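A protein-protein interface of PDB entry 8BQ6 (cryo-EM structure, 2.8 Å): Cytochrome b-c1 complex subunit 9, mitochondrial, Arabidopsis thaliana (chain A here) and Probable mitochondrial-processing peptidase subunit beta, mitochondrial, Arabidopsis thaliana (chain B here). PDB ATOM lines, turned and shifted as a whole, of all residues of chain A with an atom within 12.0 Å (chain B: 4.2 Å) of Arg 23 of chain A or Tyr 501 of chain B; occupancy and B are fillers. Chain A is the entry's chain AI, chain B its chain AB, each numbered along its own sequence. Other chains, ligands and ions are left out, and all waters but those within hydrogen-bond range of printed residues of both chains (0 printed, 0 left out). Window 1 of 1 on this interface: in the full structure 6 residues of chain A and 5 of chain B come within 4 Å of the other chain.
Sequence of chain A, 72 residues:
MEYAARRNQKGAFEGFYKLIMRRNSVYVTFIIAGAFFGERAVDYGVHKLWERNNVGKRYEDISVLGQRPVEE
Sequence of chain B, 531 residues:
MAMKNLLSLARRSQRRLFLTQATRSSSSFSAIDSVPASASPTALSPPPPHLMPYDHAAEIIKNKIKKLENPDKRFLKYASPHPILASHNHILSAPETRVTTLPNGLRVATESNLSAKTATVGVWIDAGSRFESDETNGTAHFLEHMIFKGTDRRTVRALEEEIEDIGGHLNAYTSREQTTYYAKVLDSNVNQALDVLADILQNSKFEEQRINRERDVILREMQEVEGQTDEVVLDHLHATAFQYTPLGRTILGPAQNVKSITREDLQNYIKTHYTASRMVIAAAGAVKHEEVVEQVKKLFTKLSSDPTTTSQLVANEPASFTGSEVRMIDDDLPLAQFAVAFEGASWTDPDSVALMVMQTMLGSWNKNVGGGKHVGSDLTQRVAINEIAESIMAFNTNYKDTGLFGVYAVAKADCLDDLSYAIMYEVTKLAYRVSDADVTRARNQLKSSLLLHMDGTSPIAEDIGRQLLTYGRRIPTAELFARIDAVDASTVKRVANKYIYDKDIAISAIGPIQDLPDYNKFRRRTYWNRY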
ATOM      1  N   GLU A  14      19.042   6.598  14.189  1.00  0.00           N
ATOM      2  CA  GLU A  14      18.668   6.053  15.492  1.00  0.00           C
ATOM      3  C   GLU A  14      17.335   6.601  15.989  1.00  0.00           C
ATOM      4  O   GLU A  14      16.629   5.913  16.735  1.00  0.00           O
ATOM      5  CB  GLU A  14      19.766   6.330  16.517  1.00  0.00           C
ATOM      6  CG  GLU A  14      20.130   5.124  17.375  1.00  0.00           C
ATOM      7  CD  GLU A  14      20.897   4.059  16.616  1.00  0.00           C
ATOM      8  OE1 GLU A  14      20.793   2.871  16.988  1.00  0.00           O
ATOM      9  OE2 GLU A  14      21.613   4.407  15.654  1.00  0.00           O
ATOM     10  N   GLY A  15      16.979   7.831  15.616  1.00  0.00           N
ATOM     11  CA  GLY A  15      15.670   8.346  15.987  1.00  0.00           C
ATOM     12  C   GLY A  15      14.549   7.575  15.318  1.00  0.00           C
ATOM     13  O   GLY A  15      13.506   7.309  15.922  1.00  0.00           O
ATOM     14  N   PHE A  16      14.752   7.217  14.051  1.00  0.00           N
ATOM     15  CA  PHE A  16      13.838   6.329  13.346  1.00  0.00           C
ATOM     16  C   PHE A  16      13.796   4.951  13.993  1.00  0.00           C
ATOM     17  O   PHE A  16      12.730   4.330  14.075  1.00  0.00           O
ATOM     18  CB  PHE A  16      14.285   6.233  11.890  1.00  0.00           C
ATOM     19  CG  PHE A  16      13.282   5.614  10.978  1.00  0.00           C
ATOM     20  CD1 PHE A  16      12.228   6.363  10.483  1.00  0.00           C
ATOM     21  CD2 PHE A  16      13.407   4.295  10.584  1.00  0.00           C
ATOM     22  CE1 PHE A  16      11.312   5.804   9.629  1.00  0.00           C
ATOM     23  CE2 PHE A  16      12.492   3.729   9.730  1.00  0.00           C
ATOM     24  CZ  PHE A  16      11.446   4.487   9.246  1.00  0.00           C
ATOM     25  N   TYR A  17      14.949   4.461  14.452  1.00  0.00           N
ATOM     26  CA  TYR A  17      15.023   3.153  15.094  1.00  0.00           C
ATOM     27  C   TYR A  17      14.159   3.105  16.348  1.00  0.00           C
ATOM     28  O   TYR A  17      13.536   2.082  16.652  1.00  0.00           O
ATOM     29  CB  TYR A  17      16.480   2.838  15.432  1.00  0.00           C
ATOM     30  CG  TYR A  17      16.676   1.544  16.175  1.00  0.00           C
ATOM     31  CD1 TYR A  17      16.625   1.509  17.561  1.00  0.00           C
ATOM     32  CD2 TYR A  17      16.944   0.364  15.500  1.00  0.00           C
ATOM     33  CE1 TYR A  17      16.801   0.341  18.250  1.00  0.00           C
ATOM     34  CE2 TYR A  17      17.128  -0.817  16.186  1.00  0.00           C
ATOM     35  CZ  TYR A  17      17.055  -0.819  17.563  1.00  0.00           C
ATOM     36  OH  TYR A  17      17.235  -1.982  18.269  1.00  0.00           O
ATOM     37  N   LYS A  18      14.117   4.208  17.092  1.00  0.00           N
ATOM     38  CA  LYS A  18      13.442   4.222  18.381  1.00  0.00           C
ATOM     39  C   LYS A  18      11.924   4.154  18.245  1.00  0.00           C
ATOM     40  O   LYS A  18      11.250   3.693  19.171  1.00  0.00           O
ATOM     41  CB  LYS A  18      13.885   5.471  19.146  1.00  0.00           C
ATOM     42  CG  LYS A  18      13.338   5.625  20.546  1.00  0.00           C
ATOM     43  CD  LYS A  18      13.901   6.882  21.202  1.00  0.00           C
ATOM     44  CE  LYS A  18      13.343   7.070  22.608  1.00  0.00           C
ATOM     45  NZ  LYS A  18      13.866   8.289  23.288  1.00  0.00           N
ATOM     46  N   LEU A  19      11.367   4.578  17.114  1.00  0.00           N
ATOM     47  CA  LEU A  19       9.922   4.567  16.918  1.00  0.00           C
ATOM     48  C   LEU A  19       9.412   3.301  16.245  1.00  0.00           C
ATOM     49  O   LEU A  19       8.324   2.826  16.583  1.00  0.00           O
ATOM     50  CB  LEU A  19       9.493   5.785  16.092  1.00  0.00           C
ATOM     51  CG  LEU A  19       8.836   6.912  16.892  1.00  0.00           C
ATOM     52  CD1 LEU A  19       9.879   7.655  17.705  1.00  0.00           C
ATOM     53  CD2 LEU A  19       8.084   7.868  15.980  1.00  0.00           C
ATOM     54  N   ILE A  20      10.174   2.727  15.317  1.00  0.00           N
ATOM     55  CA  ILE A  20       9.665   1.672  14.459  1.00  0.00           C
ATOM     56  C   ILE A  20      10.359   0.332  14.675  1.00  0.00           C
ATOM     57  O   ILE A  20       9.688  -0.708  14.647  1.00  0.00           O
ATOM     58  CB  ILE A  20       9.759   2.102  12.984  1.00  0.00           C
ATOM     59  CG1 ILE A  20       9.066   3.448  12.790  1.00  0.00           C
ATOM     60  CG2 ILE A  20       9.164   1.045  12.088  1.00  0.00           C
ATOM     61  CD1 ILE A  20       8.908   3.845  11.356  1.00  0.00           C
ATOM     62  N   MET A  21      11.672   0.313  14.872  1.00  0.00           N
ATOM     63  CA  MET A  21      12.413  -0.935  14.957  1.00  0.00           C
ATOM     64  C   MET A  21      12.389  -1.560  16.344  1.00  0.00           C
ATOM     65  O   MET A  21      12.779  -2.722  16.485  1.00  0.00           O
ATOM     66  CB  MET A  21      13.865  -0.715  14.531  1.00  0.00           C
ATOM     67  CG  MET A  21      14.121  -0.845  13.042  1.00  0.00           C
ATOM     68  SD  MET A  21      13.618   0.628  12.136  1.00  0.00           S
ATOM     69  CE  MET A  21      14.151   0.213  10.479  1.00  0.00           C
ATOM     70  N   ARG A  22      11.951  -0.826  17.369  1.00  0.00           N
ATOM     71  CA  ARG A  22      12.034  -1.352  18.728  1.00  0.00           C
ATOM     72  C   ARG A  22      11.182  -2.603  18.908  1.00  0.00           C
ATOM     73  O   ARG A  22      11.626  -3.563  19.549  1.00  0.00           O
ATOM     74  CB  ARG A  22      11.624  -0.279  19.736  1.00  0.00           C
ATOM     75  CG  ARG A  22      12.492  -0.241  20.985  1.00  0.00           C
ATOM     76  CD  ARG A  22      11.709   0.259  22.186  1.00  0.00           C
ATOM     77  NE  ARG A  22      10.728   1.271  21.813  1.00  0.00           N
ATOM     78  CZ  ARG A  22      10.979   2.572  21.773  1.00  0.00           C
ATOM     79  NH1 ARG A  22      12.161   3.059  22.110  1.00  0.00           N
ATOM     80  NH2 ARG A  22      10.022   3.405  21.373  1.00  0.00           N
ATOM     81  N   ARG A  23       9.971  -2.618  18.360  1.00  0.00           N
ATOM     82  CA  ARG A  23       9.083  -3.768  18.445  1.00  0.00           C
ATOM     83  C   ARG A  23       8.905  -4.364  17.058  1.00  0.00           C
ATOM     84  O   ARG A  23       8.690  -3.636  16.084  1.00  0.00           O
ATOM     85  CB  ARG A  23       7.715  -3.381  19.023  1.00  0.00           C
ATOM     86  CG  ARG A  23       7.700  -3.189  20.531  1.00  0.00           C
ATOM     87  CD  ARG A  23       7.459  -4.499  21.267  1.00  0.00           C
ATOM     88  NE  ARG A  23       8.169  -4.528  22.539  1.00  0.00           N
ATOM     89  CZ  ARG A  23       9.472  -4.745  22.660  1.00  0.00           C
ATOM     90  NH1 ARG A  23      10.230  -4.997  21.606  1.00  0.00           N
ATOM     91  NH2 ARG A  23      10.027  -4.706  23.867  1.00  0.00           N
ATOM     92  N   ASN A  24       8.996  -5.694  16.975  1.00  0.00           N
ATOM     93  CA  ASN A  24       8.820  -6.367  15.694  1.00  0.00           C
ATOM     94  C   ASN A  24       7.424  -6.150  15.126  1.00  0.00           C
ATOM     95  O   ASN A  24       7.266  -6.043  13.905  1.00  0.00           O
ATOM     96  CB  ASN A  24       9.105  -7.859  15.839  1.00  0.00           C
ATOM     97  CG  ASN A  24       9.506  -8.499  14.530  1.00  0.00           C
ATOM     98  OD1 ASN A  24      10.290  -7.937  13.768  1.00  0.00           O
ATOM     99  ND2 ASN A  24       8.969  -9.683  14.261  1.00  0.00           N
ATOM    100  N   SER A  25       6.405  -6.077  15.985  1.00  0.00           N
ATOM    101  CA  SER A  25       5.039  -5.903  15.501  1.00  0.00           C
ATOM    102  C   SER A  25       4.888  -4.593  14.737  1.00  0.00           C
ATOM    103  O   SER A  25       4.208  -4.534  13.707  1.00  0.00           O
ATOM    104  CB  SER A  25       4.060  -5.962  16.672  1.00  0.00           C
ATOM    105  OG  SER A  25       4.570  -5.262  17.794  1.00  0.00           O
ATOM    106  N   VAL A  26       5.506  -3.524  15.241  1.00  0.00           N
ATOM    107  CA  VAL A  26       5.513  -2.255  14.521  1.00  0.00           C
ATOM    108  C   VAL A  26       6.375  -2.356  13.271  1.00  0.00           C
ATOM    109  O   VAL A  26       5.996  -1.879  12.195  1.00  0.00           O
ATOM    110  CB  VAL A  26       5.986  -1.128  15.453  1.00  0.00           C
ATOM    111  CG1 VAL A  26       6.024   0.193  14.719  1.00  0.00           C
ATOM    112  CG2 VAL A  26       5.060  -1.038  16.648  1.00  0.00           C
ATOM    113  N   TYR A  27       7.545  -2.984  13.395  1.00  0.00           N
ATOM    114  CA  TYR A  27       8.447  -3.107  12.257  1.00  0.00           C
ATOM    115  C   TYR A  27       7.837  -3.970  11.161  1.00  0.00           C
ATOM    116  O   TYR A  27       8.128  -3.779   9.975  1.00  0.00           O
ATOM    117  CB  TYR A  27       9.782  -3.679  12.721  1.00  0.00           C
ATOM    118  CG  TYR A  27      10.775  -3.892  11.614  1.00  0.00           C
ATOM    119  CD1 TYR A  27      11.313  -2.818  10.927  1.00  0.00           C
ATOM    120  CD2 TYR A  27      11.183  -5.167  11.262  1.00  0.00           C
ATOM    121  CE1 TYR A  27      12.224  -3.008   9.918  1.00  0.00           C
ATOM    122  CE2 TYR A  27      12.095  -5.366  10.259  1.00  0.00           C
ATOM    123  CZ  TYR A  27      12.611  -4.284   9.589  1.00  0.00           C
ATOM    124  OH  TYR A  27      13.521  -4.484   8.581  1.00  0.00           O
ATOM    125  N   VAL A  28       6.989  -4.928  11.536  1.00  0.00           N
ATOM    126  CA  VAL A  28       6.271  -5.693  10.524  1.00  0.00           C
ATOM    127  C   VAL A  28       5.230  -4.816   9.838  1.00  0.00           C
ATOM    128  O   VAL A  28       5.097  -4.841   8.611  1.00  0.00           O
ATOM    129  CB  VAL A  28       5.653  -6.959  11.141  1.00  0.00           C
ATOM    130  CG1 VAL A  28       4.631  -7.554  10.201  1.00  0.00           C
ATOM    131  CG2 VAL A  28       6.739  -7.981  11.423  1.00  0.00           C
ATOM    132  N   THR A  29       4.495  -4.009  10.611  1.00  0.00           N
ATOM    133  CA  THR A  29       3.529  -3.085  10.017  1.00  0.00           C
ATOM    134  C   THR A  29       4.222  -2.045   9.152  1.00  0.00           C
ATOM    135  O   THR A  29       3.641  -1.532   8.188  1.00  0.00           O
ATOM    136  CB  THR A  29       2.714  -2.393  11.111  1.00  0.00           C
ATOM    137  OG1 THR A  29       2.198  -3.374  12.016  1.00  0.00           O
ATOM    138  CG2 THR A  29       1.555  -1.611  10.505  1.00  0.00           C
ATOM    139  N   PHE A  30       5.457  -1.696   9.502  1.00  0.00           N
ATOM    140  CA  PHE A  30       6.235  -0.789   8.673  1.00  0.00           C
ATOM    141  C   PHE A  30       6.564  -1.419   7.325  1.00  0.00           C
ATOM    142  O   PHE A  30       6.583  -0.733   6.296  1.00  0.00           O
ATOM    143  CB  PHE A  30       7.502  -0.397   9.422  1.00  0.00           C
ATOM    144  CG  PHE A  30       8.436   0.456   8.635  1.00  0.00           C
ATOM    145  CD1 PHE A  30       8.057   1.714   8.212  1.00  0.00           C
ATOM    146  CD2 PHE A  30       9.701  -0.001   8.320  1.00  0.00           C
ATOM    147  CE1 PHE A  30       8.920   2.500   7.489  1.00  0.00           C
ATOM    148  CE2 PHE A  30      10.571   0.785   7.597  1.00  0.00           C
ATOM    149  CZ  PHE A  30      10.179   2.038   7.180  1.00  0.00           C
ATOM    150  N   ILE A  31       6.839  -2.722   7.308  1.00  0.00           N
ATOM    151  CA  ILE A  31       7.173  -3.377   6.048  1.00  0.00           C
ATOM    152  C   ILE A  31       5.920  -3.582   5.203  1.00  0.00           C
ATOM    153  O   ILE A  31       5.968  -3.511   3.969  1.00  0.00           O
ATOM    154  CB  ILE A  31       7.930  -4.691   6.318  1.00  0.00           C
ATOM    155  CG1 ILE A  31       9.351  -4.358   6.772  1.00  0.00           C
ATOM    156  CG2 ILE A  31       7.986  -5.563   5.076  1.00  0.00           C
ATOM    157  CD1 ILE A  31      10.071  -5.492   7.433  1.00  0.00           C
ATOM    158  N   ILE A  32       4.776  -3.814   5.848  1.00  0.00           N
ATOM    159  CA  ILE A  32       3.527  -3.960   5.103  1.00  0.00           C
ATOM    160  C   ILE A  32       3.096  -2.617   4.521  1.00  0.00           C
ATOM    161  O   ILE A  32       2.651  -2.534   3.370  1.00  0.00           O
ATOM    162  CB  ILE A  32       2.438  -4.580   5.997  1.00  0.00           C
ATOM    163  CG1 ILE A  32       2.984  -5.825   6.699  1.00  0.00           C
ATOM    164  CG2 ILE A  32       1.203  -4.927   5.189  1.00  0.00           C
ATOM    165  CD1 ILE A  32       3.070  -7.052   5.819  1.00  0.00           C
ATOM    166  N   TYR B 432      11.778  -7.899  28.890  1.00  0.00           N
ATOM    167  CA  TYR B 432      10.374  -8.163  28.602  1.00  0.00           C
ATOM    168  C   TYR B 432       9.559  -8.515  29.835  1.00  0.00           C
ATOM    169  O   TYR B 432       8.561  -7.847  30.119  1.00  0.00           O
ATOM    170  CB  TYR B 432      10.265  -9.296  27.575  1.00  0.00           C
ATOM    171  CG  TYR B 432      10.888  -8.985  26.237  1.00  0.00           C
ATOM    172  CD1 TYR B 432      10.224  -8.203  25.305  1.00  0.00           C
ATOM    173  CD2 TYR B 432      12.141  -9.477  25.906  1.00  0.00           C
ATOM    174  CE1 TYR B 432      10.791  -7.925  24.079  1.00  0.00           C
ATOM    175  CE2 TYR B 432      12.715  -9.204  24.687  1.00  0.00           C
ATOM    176  CZ  TYR B 432      12.039  -8.428  23.778  1.00  0.00           C
ATOM    177  OH  TYR B 432      12.615  -8.159  22.562  1.00  0.00           O
ATOM    178  N   ALA B 496      17.461  -2.694  31.316  1.00  0.00           N
ATOM    179  CA  ALA B 496      17.803  -3.787  30.411  1.00  0.00           C
ATOM    180  C   ALA B 496      17.576  -3.395  28.957  1.00  0.00           C
ATOM    181  O   ALA B 496      18.336  -3.799  28.070  1.00  0.00           O
ATOM    182  CB  ALA B 496      16.991  -5.031  30.760  1.00  0.00           C
ATOM    183  N   ASN B 497      16.521  -2.624  28.692  1.00  0.00           N
ATOM    184  CA  ASN B 497      16.270  -2.156  27.335  1.00  0.00           C
ATOM    185  C   ASN B 497      17.341  -1.180  26.876  1.00  0.00           C
ATOM    186  O   ASN B 497      17.564  -1.023  25.672  1.00  0.00           O
ATOM    187  CB  ASN B 497      14.895  -1.505  27.261  1.00  0.00           C
ATOM    188  CG  ASN B 497      13.825  -2.471  26.828  1.00  0.00           C
ATOM    189  OD1 ASN B 497      13.696  -2.781  25.648  1.00  0.00           O
ATOM    190  ND2 ASN B 497      13.069  -2.978  27.787  1.00  0.00           N
ATOM    191  N   TYR B 499      20.627  -1.458  27.932  1.00  0.00           N
ATOM    192  CA  TYR B 499      21.930  -2.112  27.904  1.00  0.00           C
ATOM    193  C   TYR B 499      21.947  -3.481  27.244  1.00  0.00           C
ATOM    194  O   TYR B 499      23.003  -3.898  26.769  1.00  0.00           O
ATOM    195  CB  TYR B 499      22.480  -2.265  29.327  1.00  0.00           C
ATOM    196  CG  TYR B 499      22.847  -0.959  29.972  1.00  0.00           C
ATOM    197  CD1 TYR B 499      24.044  -0.328  29.676  1.00  0.00           C
ATOM    198  CD2 TYR B 499      21.993  -0.354  30.877  1.00  0.00           C
ATOM    199  CE1 TYR B 499      24.377   0.868  30.261  1.00  0.00           C
ATOM    200  CE2 TYR B 499      22.316   0.838  31.467  1.00  0.00           C
ATOM    201  CZ  TYR B 499      23.507   1.446  31.158  1.00  0.00           C
ATOM    202  OH  TYR B 499      23.823   2.640  31.754  1.00  0.00           O
ATOM    203  N   ILE B 500      20.828  -4.195  27.208  1.00  0.00           N
ATOM    204  CA  ILE B 500      20.793  -5.585  26.771  1.00  0.00           C
ATOM    205  C   ILE B 500      20.079  -5.740  25.433  1.00  0.00           C
ATOM    206  O   ILE B 500      20.526  -6.489  24.564  1.00  0.00           O
ATOM    207  CB  ILE B 500      20.152  -6.487  27.851  1.00  0.00           C
ATOM    208  CG1 ILE B 500      21.171  -6.831  28.933  1.00  0.00           C
ATOM    209  CG2 ILE B 500      19.563  -7.748  27.244  1.00  0.00           C
ATOM    210  CD1 ILE B 500      20.577  -6.890  30.309  1.00  0.00           C
ATOM    211  N   TYR B 501      18.967  -5.039  25.250  1.00  0.00           N
ATOM    212  CA  TYR B 501      18.112  -5.300  24.102  1.00  0.00           C
ATOM    213  C   TYR B 501      18.759  -4.827  22.804  1.00  0.00           C
ATOM    214  O   TYR B 501      19.070  -3.644  22.647  1.00  0.00           O
ATOM    215  CB  TYR B 501      16.759  -4.622  24.305  1.00  0.00           C
ATOM    216  CG  TYR B 501      15.894  -4.672  23.083  1.00  0.00           C
ATOM    217  CD1 TYR B 501      15.151  -5.801  22.783  1.00  0.00           C
ATOM    218  CD2 TYR B 501      15.833  -3.597  22.216  1.00  0.00           C
ATOM    219  CE1 TYR B 501      14.369  -5.849  21.658  1.00  0.00           C
ATOM    220  CE2 TYR B 501      15.060  -3.638  21.093  1.00  0.00           C
ATOM    221  CZ  TYR B 501      14.329  -4.765  20.814  1.00  0.00           C
ATOM    222  OH  TYR B 501      13.551  -4.798  19.685  1.00  0.00           O
ATOM    223  N   ASP B 502      18.950  -5.764  21.869  1.00  0.00           N
ATOM    224  CA  ASP B 502      19.444  -5.473  20.519  1.00  0.00           C
ATOM    225  C   ASP B 502      20.786  -4.744  20.551  1.00  0.00           C
ATOM    226  O   ASP B 502      20.994  -3.742  19.864  1.00  0.00           O
ATOM    227  CB  ASP B 502      18.410  -4.673  19.722  1.00  0.00           C
ATOM    228  CG  ASP B 502      18.585  -4.815  18.219  1.00  0.00           C
ATOM    229  OD1 ASP B 502      19.447  -5.600  17.779  1.00  0.00           O
ATOM    230  OD2 ASP B 502      17.867  -4.122  17.473  1.00  0.00           O
ATOM    231  N   LYS B 503      21.714  -5.268  21.345  1.00  0.00           N
ATOM    232  CA  LYS B 503      22.996  -4.618  21.574  1.00  0.00           C
ATOM    233  C   LYS B 503      24.142  -5.544  21.190  1.00  0.00           C
ATOM    234  O   LYS B 503      24.033  -6.769  21.295  1.00  0.00           O
ATOM    235  CB  LYS B 503      23.137  -4.199  23.037  1.00  0.00           C
ATOM    236  CG  LYS B 503      23.269  -2.713  23.250  1.00  0.00           C
ATOM    237  CD  LYS B 503      22.031  -1.972  22.797  1.00  0.00           C
ATOM    238  CE  LYS B 503      22.107  -0.527  23.220  1.00  0.00           C
ATOM    239  NZ  LYS B 503      23.391   0.080  22.790  1.00  0.00           N
ATOM    240  N   THR B 526      19.653 -11.472  21.236  1.00  0.00           N
ATOM    241  CA  THR B 526      19.508 -10.334  22.133  1.00  0.00           C
ATOM    242  C   THR B 526      18.138  -9.676  22.044  1.00  0.00           C
ATOM    243  O   THR B 526      17.868  -8.741  22.804  1.00  0.00           O
ATOM    244  CB  THR B 526      20.592  -9.282  21.855  1.00  0.00           C
ATOM    245  OG1 THR B 526      20.477  -8.813  20.507  1.00  0.00           O
ATOM    246  CG2 THR B 526      21.979  -9.862  22.071  1.00  0.00           C
ATOM    247  N   TYR B 527      17.272 -10.133  21.145  1.00  0.00           N
ATOM    248  CA  TYR B 527      15.919  -9.610  21.045  1.00  0.00           C
ATOM    249  C   TYR B 527      14.969 -10.757  20.740  1.00  0.00           C
ATOM    250  O   TYR B 527      15.373 -11.820  20.260  1.00  0.00           O
ATOM    251  CB  TYR B 527      15.812  -8.511  19.978  1.00  0.00           C
ATOM    252  CG  TYR B 527      16.395  -8.890  18.641  1.00  0.00           C
ATOM    253  CD1 TYR B 527      17.724  -8.628  18.347  1.00  0.00           C
ATOM    254  CD2 TYR B 527      15.620  -9.509  17.672  1.00  0.00           C
ATOM    255  CE1 TYR B 527      18.266  -8.973  17.135  1.00  0.00           C
ATOM    256  CE2 TYR B 527      16.154  -9.857  16.454  1.00  0.00           C
ATOM    257  CZ  TYR B 527      17.479  -9.585  16.191  1.00  0.00           C
ATOM    258  OH  TYR B 527      18.024  -9.928  14.979  1.00  0.00           O
ATOM    259  N   TYR B 531       7.590 -10.084  19.933  1.00  0.00           N
ATOM    260  CA  TYR B 531       7.104  -8.910  20.643  1.00  0.00           C
ATOM    261  C   TYR B 531       7.250  -7.656  19.788  1.00  0.00           C
ATOM    262  O   TYR B 531       6.963  -7.668  18.592  1.00  0.00           O
ATOM    263  CB  TYR B 531       7.858  -8.734  21.958  1.00  0.00           C
ATOM    264  CG  TYR B 531       7.394  -9.643  23.069  1.00  0.00           C
ATOM    265  CD1 TYR B 531       6.089  -9.594  23.534  1.00  0.00           C
ATOM    266  CD2 TYR B 531       8.264 -10.550  23.656  1.00  0.00           C
ATOM    267  CE1 TYR B 531       5.665 -10.423  24.554  1.00  0.00           C
ATOM    268  CE2 TYR B 531       7.849 -11.380  24.675  1.00  0.00           C
ATOM    269  CZ  TYR B 531       6.551 -11.314  25.119  1.00  0.00           C
ATOM    270  OH  TYR B 531       6.140 -12.145  26.133  1.00  0.00           O
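N of Arg 22 of chain A lies within hydrogen-bond range of O of Tyr 17 of chain A, 3.4 Å away. The backbone carbonyl oxygen of Ser 25 of chain A sits at hydrogen-bond distance from the side-chain hydroxyl of Thr 29 of chain A. The backbone carbonyl oxygen (O) of Ala 496 of chain B is in hydrogen-bond range of the backbone NH (N) of Tyr 501 of chain B (3.1 Å). N of Asp 502 of chain B sits at hydrogen-bond distance from O of Thr 526 of chain B (3.3 Å). The backbone carbonyl oxygen (O) of Lys 18 of chain A sits at hydrogen-bond distance from the guanidinium group (NH2) of Arg 22 of chain A (2.5 Å).
Among the printed residues, pairs that only touch across the chains: Arg 23 of chain A with Tyr 432 of chain B (3.3 Å), Arg 23 of chain A with Tyr 531 of chain B (3.5 Å), Arg 23 of chain A with Tyr 501 of chain B (3.8 Å), Met 21 of chain A with Tyr 501 of chain B (3.9 Å) and Tyr 17 of chain A with Tyr 501 of chain B (3.9 Å).
O of Tyr 531 of chain B is in hydrogen-bond range of N of Asn 24 of chain A, 3.3 Å away. OH of Tyr 17 of chain A sits close to OD2 of Asp 502 of chain B, at 2.4 Å. OH of Tyr 501 of chain B lies close to O of Arg 22 of chain A (2.3 Å). N of Ser 25 of chain A sits at hydrogen-bond distance from O of Tyr 531 of chain B (3.1 Å).
Of the 19 printed residues of chain A, 6 touch a printed residue of chain B. Hydrophobic or aromatic side chains of chain A within 4 Å of the printed part of chain B: Tyr 17. Of the 11 printed residues of chain B, 4 touch a printed residue of chain A. Hydrophobic or aromatic side chains of chain B that line the printed part of chain A: Tyr 432 and Tyr 501. Along chain B the printed residues that touch a printed residue of chain A span positions 432 to 531. Among the printed residues, no Asp or Glu carboxylate lies within 4 Å of a Lys or Arg side-chain nitrogen of the other chain.
Printed residues of chain B within 4 Å of Tyr 17 of chain A: Tyr 501 and Asp 502. Printed residues of chain B within 4 Å of Met 21 of chain A: Tyr 501. Of the printed residues of chain B, Arg 22 of chain A touches Tyr 501. Arg 23 of chain A touches just these residues of chain B: Tyr 432 (3.3 Å), Tyr 501 (3.8 Å) and Tyr 531 (3.5 Å). Of the printed residues of chain B, Asn 24 of chain A touches Tyr 531. Of the printed residues of chain B, Ser 25 of chain A touches Tyr 531 (3.1 Å). Phe 30 of chain A touches none of the printed residues of chain B. Of chain A, only Arg 23 (3.3 Å) comes within 4 Å of Tyr 432 of chain B. No residue of chain A comes within 4 Å of Asn 497 of chain B. Ile 500 of chain B touches none of the printed residues of chain A. Of chain A, only Tyr 17, Met 21, Arg 22 and Arg 23 come within 4 Å of Tyr 501 of chain B. Of chain A, only Tyr 17 comes within 4 Å of Asp 502 of chain B.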
